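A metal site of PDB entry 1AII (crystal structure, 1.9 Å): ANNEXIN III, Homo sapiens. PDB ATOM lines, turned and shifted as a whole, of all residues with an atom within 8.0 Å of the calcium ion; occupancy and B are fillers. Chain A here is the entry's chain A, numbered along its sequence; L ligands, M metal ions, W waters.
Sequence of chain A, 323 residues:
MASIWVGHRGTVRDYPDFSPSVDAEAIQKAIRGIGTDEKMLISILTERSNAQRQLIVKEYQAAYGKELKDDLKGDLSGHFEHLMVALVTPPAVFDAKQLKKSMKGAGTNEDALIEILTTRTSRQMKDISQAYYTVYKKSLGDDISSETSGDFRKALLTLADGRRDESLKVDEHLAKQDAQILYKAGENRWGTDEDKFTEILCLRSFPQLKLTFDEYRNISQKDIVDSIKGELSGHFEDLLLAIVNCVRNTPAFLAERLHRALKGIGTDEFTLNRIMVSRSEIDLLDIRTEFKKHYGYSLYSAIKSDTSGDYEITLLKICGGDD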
ATOM      1  N   LEU A 182      19.094 -18.826  -5.819  1.00  0.00           N
ATOM      2  CA  LEU A 182      18.118 -18.884  -4.720  1.00  0.00           C
ATOM      3  C   LEU A 182      17.150 -20.043  -4.991  1.00  0.00           C
ATOM      4  O   LEU A 182      16.771 -20.828  -4.130  1.00  0.00           O
ATOM      5  CB  LEU A 182      17.349 -17.573  -4.584  1.00  0.00           C
ATOM      6  CG  LEU A 182      18.030 -16.352  -3.929  1.00  0.00           C
ATOM      7  CD1 LEU A 182      17.074 -15.168  -3.863  1.00  0.00           C
ATOM      8  CD2 LEU A 182      18.565 -16.684  -2.545  1.00  0.00           C
ATOM      9  N   TYR A 183      16.693 -20.139  -6.232  1.00  0.00           N
ATOM     10  CA  TYR A 183      15.767 -21.185  -6.661  1.00  0.00           C
ATOM     11  C   TYR A 183      16.388 -22.566  -6.446  1.00  0.00           C
ATOM     12  O   TYR A 183      15.712 -23.452  -5.914  1.00  0.00           O
ATOM     13  CB  TYR A 183      15.335 -21.019  -8.113  1.00  0.00           C
ATOM     14  CG  TYR A 183      14.283 -22.003  -8.563  1.00  0.00           C
ATOM     15  CD1 TYR A 183      12.961 -21.889  -8.127  1.00  0.00           C
ATOM     16  CD2 TYR A 183      14.585 -23.042  -9.434  1.00  0.00           C
ATOM     17  CE1 TYR A 183      11.994 -22.776  -8.541  1.00  0.00           C
ATOM     18  CE2 TYR A 183      13.622 -23.952  -9.846  1.00  0.00           C
ATOM     19  CZ  TYR A 183      12.322 -23.819  -9.396  1.00  0.00           C
ATOM     20  OH  TYR A 183      11.364 -24.724  -9.802  1.00  0.00           O
ATOM     21  N   LYS A 184      17.628 -22.788  -6.821  1.00  0.00           N
ATOM     22  CA  LYS A 184      18.319 -24.054  -6.666  1.00  0.00           C
ATOM     23  C   LYS A 184      18.594 -24.364  -5.200  1.00  0.00           C
ATOM     24  O   LYS A 184      18.614 -25.536  -4.829  1.00  0.00           O
ATOM     25  CB  LYS A 184      19.680 -24.091  -7.379  1.00  0.00           C
ATOM     26  CG  LYS A 184      19.596 -24.174  -8.890  1.00  0.00           C
ATOM     27  CD  LYS A 184      20.963 -24.365  -9.550  1.00  0.00           C
ATOM     28  CE  LYS A 184      20.901 -23.961 -11.013  1.00  0.00           C
ATOM     29  NZ  LYS A 184      22.228 -23.530 -11.558  1.00  0.00           N
ATOM     30  N   ALA A 185      18.815 -23.322  -4.400  1.00  0.00           N
ATOM     31  CA  ALA A 185      19.106 -23.456  -2.991  1.00  0.00           C
ATOM     32  C   ALA A 185      17.934 -23.805  -2.087  1.00  0.00           C
ATOM     33  O   ALA A 185      18.115 -24.268  -0.962  1.00  0.00           O
ATOM     34  CB  ALA A 185      19.666 -22.097  -2.501  1.00  0.00           C
ATOM     35  N   GLY A 186      16.736 -23.571  -2.567  1.00  0.00           N
ATOM     36  CA  GLY A 186      15.509 -23.800  -1.861  1.00  0.00           C
ATOM     37  C   GLY A 186      14.493 -24.602  -2.644  1.00  0.00           C
ATOM     38  O   GLY A 186      14.559 -25.817  -2.601  1.00  0.00           O
ATOM     39  N   GLU A 187      13.567 -24.033  -3.356  1.00  0.00           N
ATOM     40  CA  GLU A 187      12.543 -24.711  -4.103  1.00  0.00           C
ATOM     41  C   GLU A 187      12.975 -25.933  -4.882  1.00  0.00           C
ATOM     42  O   GLU A 187      12.298 -26.950  -4.810  1.00  0.00           O
ATOM     43  CB  GLU A 187      11.870 -23.749  -5.112  1.00  0.00           C
ATOM     44  CG  GLU A 187      11.121 -22.617  -4.446  1.00  0.00           C
ATOM     45  CD  GLU A 187       9.832 -23.019  -3.756  1.00  0.00           C
ATOM     46  OE1 GLU A 187       9.330 -24.151  -3.895  1.00  0.00           O
ATOM     47  OE2 GLU A 187       9.244 -22.191  -3.053  1.00  0.00           O
ATOM     48  N   ASN A 188      14.057 -25.837  -5.639  1.00  0.00           N
ATOM     49  CA  ASN A 188      14.517 -26.940  -6.450  1.00  0.00           C
ATOM     50  C   ASN A 188      15.218 -28.082  -5.761  1.00  0.00           C
ATOM     51  O   ASN A 188      15.581 -29.030  -6.483  1.00  0.00           O
ATOM     52  CB  ASN A 188      15.430 -26.352  -7.550  1.00  0.00           C
ATOM     53  CG  ASN A 188      15.469 -27.241  -8.793  1.00  0.00           C
ATOM     54  OD1 ASN A 188      16.559 -27.684  -9.169  1.00  0.00           O
ATOM     55  ND2 ASN A 188      14.305 -27.494  -9.379  1.00  0.00           N
ATOM     56  N   ARG A 189      15.444 -28.112  -4.468  1.00  0.00           N
ATOM     57  CA  ARG A 189      16.129 -29.279  -3.912  1.00  0.00           C
ATOM     58  C   ARG A 189      15.472 -29.801  -2.664  1.00  0.00           C
ATOM     59  O   ARG A 189      14.640 -29.076  -2.146  1.00  0.00           O
ATOM     60  CB  ARG A 189      17.563 -28.874  -3.533  1.00  0.00           C
ATOM     61  CG  ARG A 189      17.665 -27.649  -2.637  1.00  0.00           C
ATOM     62  CD  ARG A 189      19.051 -27.570  -2.034  1.00  0.00           C
ATOM     63  NE  ARG A 189      19.171 -28.434  -0.869  1.00  0.00           N
ATOM     64  CZ  ARG A 189      20.244 -28.637  -0.127  1.00  0.00           C
ATOM     65  NH1 ARG A 189      21.394 -28.028  -0.408  1.00  0.00           N
ATOM     66  NH2 ARG A 189      20.196 -29.461   0.916  1.00  0.00           N
ATOM     67  N   TRP A 190      15.808 -30.979  -2.173  1.00  0.00           N
ATOM     68  CA  TRP A 190      15.217 -31.474  -0.937  1.00  0.00           C
ATOM     69  C   TRP A 190      15.933 -30.645   0.148  1.00  0.00           C
ATOM     70  O   TRP A 190      17.146 -30.434   0.011  1.00  0.00           O
ATOM     71  CB  TRP A 190      15.468 -32.972  -0.713  1.00  0.00           C
ATOM     72  CG  TRP A 190      14.772 -33.846  -1.714  1.00  0.00           C
ATOM     73  CD1 TRP A 190      13.736 -33.526  -2.525  1.00  0.00           C
ATOM     74  CD2 TRP A 190      15.085 -35.219  -1.989  1.00  0.00           C
ATOM     75  NE1 TRP A 190      13.393 -34.592  -3.304  1.00  0.00           N
ATOM     76  CE2 TRP A 190      14.209 -35.644  -2.987  1.00  0.00           C
ATOM     77  CE3 TRP A 190      16.047 -36.100  -1.474  1.00  0.00           C
ATOM     78  CZ2 TRP A 190      14.231 -36.945  -3.518  1.00  0.00           C
ATOM     79  CZ3 TRP A 190      16.067 -37.382  -1.989  1.00  0.00           C
ATOM     80  CH2 TRP A 190      15.168 -37.792  -2.982  1.00  0.00           C
ATOM     81  N   GLY A 191      15.241 -30.193   1.206  1.00  0.00           N
ATOM     82  CA  GLY A 191      16.002 -29.382   2.138  1.00  0.00           C
ATOM     83  C   GLY A 191      16.276 -27.997   1.609  1.00  0.00           C
ATOM     84  O   GLY A 191      15.656 -27.550   0.641  1.00  0.00           O
ATOM     85  N   THR A 192      17.212 -27.295   2.220  1.00  0.00           N
ATOM     86  CA  THR A 192      17.549 -25.948   1.798  1.00  0.00           C
ATOM     87  C   THR A 192      19.014 -25.612   2.032  1.00  0.00           C
ATOM     88  O   THR A 192      19.598 -26.053   3.021  1.00  0.00           O
ATOM     89  CB  THR A 192      16.725 -24.891   2.584  1.00  0.00           C
ATOM     90  OG1 THR A 192      15.356 -25.273   2.606  1.00  0.00           O
ATOM     91  CG2 THR A 192      16.884 -23.510   1.963  1.00  0.00           C
ATOM     92  N   ASP A 193      19.617 -24.875   1.123  1.00  0.00           N
ATOM     93  CA  ASP A 193      20.976 -24.409   1.353  1.00  0.00           C
ATOM     94  C   ASP A 193      20.887 -23.045   2.029  1.00  0.00           C
ATOM     95  O   ASP A 193      21.068 -22.021   1.380  1.00  0.00           O
ATOM     96  CB  ASP A 193      21.788 -24.362   0.052  1.00  0.00           C
ATOM     97  CG  ASP A 193      23.250 -24.024   0.316  1.00  0.00           C
ATOM     98  OD1 ASP A 193      23.570 -23.637   1.468  1.00  0.00           O
ATOM     99  OD2 ASP A 193      24.067 -24.132  -0.614  1.00  0.00           O
ATOM    100  N   PHE A 197      21.070 -18.572   1.078  1.00  0.00           N
ATOM    101  CA  PHE A 197      20.023 -17.580   1.314  1.00  0.00           C
ATOM    102  C   PHE A 197      20.649 -16.414   2.087  1.00  0.00           C
ATOM    103  O   PHE A 197      20.460 -15.254   1.760  1.00  0.00           O
ATOM    104  CB  PHE A 197      18.813 -18.143   2.068  1.00  0.00           C
ATOM    105  CG  PHE A 197      17.746 -18.711   1.168  1.00  0.00           C
ATOM    106  CD1 PHE A 197      17.850 -19.987   0.631  1.00  0.00           C
ATOM    107  CD2 PHE A 197      16.627 -17.954   0.829  1.00  0.00           C
ATOM    108  CE1 PHE A 197      16.850 -20.473  -0.193  1.00  0.00           C
ATOM    109  CE2 PHE A 197      15.635 -18.439  -0.002  1.00  0.00           C
ATOM    110  CZ  PHE A 197      15.741 -19.704  -0.519  1.00  0.00           C
ATOM    111  N   SER A 227       8.684 -18.594  -0.897  1.00  0.00           N
ATOM    112  CA  SER A 227       9.736 -19.611  -0.844  1.00  0.00           C
ATOM    113  C   SER A 227      10.379 -19.624   0.535  1.00  0.00           C
ATOM    114  O   SER A 227      10.673 -20.676   1.099  1.00  0.00           O
ATOM    115  CB  SER A 227      10.779 -19.421  -1.939  1.00  0.00           C
ATOM    116  OG  SER A 227      10.224 -19.603  -3.231  1.00  0.00           O
ATOM    117  N   GLY A 230       8.094 -21.322   2.750  1.00  0.00           N
ATOM    118  CA  GLY A 230       7.927 -22.760   2.672  1.00  0.00           C
ATOM    119  C   GLY A 230       9.209 -23.507   2.943  1.00  0.00           C
ATOM    120  O   GLY A 230       9.189 -24.708   3.248  1.00  0.00           O
ATOM    121  N   GLU A 231      10.341 -22.811   2.856  1.00  0.00           N
ATOM    122  CA  GLU A 231      11.650 -23.434   3.031  1.00  0.00           C
ATOM    123  C   GLU A 231      12.223 -23.310   4.435  1.00  0.00           C
ATOM    124  O   GLU A 231      12.843 -24.236   4.953  1.00  0.00           O
ATOM    125  CB  GLU A 231      12.684 -22.813   2.100  1.00  0.00           C
ATOM    126  CG  GLU A 231      12.436 -23.074   0.637  1.00  0.00           C
ATOM    127  CD  GLU A 231      12.742 -24.506   0.251  1.00  0.00           C
ATOM    128  OE1 GLU A 231      13.780 -25.032   0.692  1.00  0.00           O
ATOM    129  OE2 GLU A 231      11.931 -25.104  -0.496  1.00  0.00           O
ATOM    130  N   LEU A 232      12.038 -22.162   5.065  1.00  0.00           N
ATOM    131  CA  LEU A 232      12.642 -21.937   6.373  1.00  0.00           C
ATOM    132  C   LEU A 232      11.593 -21.801   7.466  1.00  0.00           C
ATOM    133  O   LEU A 232      10.398 -21.855   7.214  1.00  0.00           O
ATOM    134  CB  LEU A 232      13.551 -20.720   6.276  1.00  0.00           C
ATOM    135  CG  LEU A 232      14.403 -20.629   4.998  1.00  0.00           C
ATOM    136  CD1 LEU A 232      14.710 -19.178   4.645  1.00  0.00           C
ATOM    137  CD2 LEU A 232      15.682 -21.426   5.148  1.00  0.00           C
HETATM  138  C1  LIG L   1      17.722 -29.755   4.723  1.00  0.00           C
HETATM  139  N1  LIG L   1      18.828 -30.564   4.135  1.00  0.00           N
HETATM  140  C2  LIG L   1      16.978 -30.520   5.789  1.00  0.00           C
HETATM  141  O1  LIG L   1      17.782 -31.601   6.231  1.00  0.00           O
HETATM  142 CA    CA M   1      13.632 -27.271  -0.628  1.00  0.00          CA
HETATM  143  O   HOH W   1      12.431 -28.304   1.532  1.00  0.00           O
HETATM  144  O   HOH W   2      11.631 -28.087  -2.259  1.00  0.00           O
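The side-chain hydroxyl (OG1) of Thr 192 sits close to the side-chain carboxylate (OE1) of Glu 231, at 2.5 Å.
The side-chain carboxylate (OE2) of Glu 231 sits close to the backbone NH (N) of Glu 187, at 3.5 Å.
Within 4 Å of the calcium ion: Gly 186, Arg 189, Gly 191 and Glu 231.
The nearest printed residue that does not touch the calcium ion is Trp 190 (4.2 Å).
The calcium ion is bound by the backbone carbonyl oxygen (O) of Gly 191 (2.4 Å), the backbone carbonyl oxygen (O) of Arg 189 (2.6 Å), the side-chain carboxylate (OE1) of Glu 231 (2.6 Å), the backbone carbonyl oxygen (O) of Gly 186 (2.6 Å), water W1 (2.7 Å), water W2 (2.7 Å) and the side-chain carboxylate (OE2) of Glu 231 (2.8 Å).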
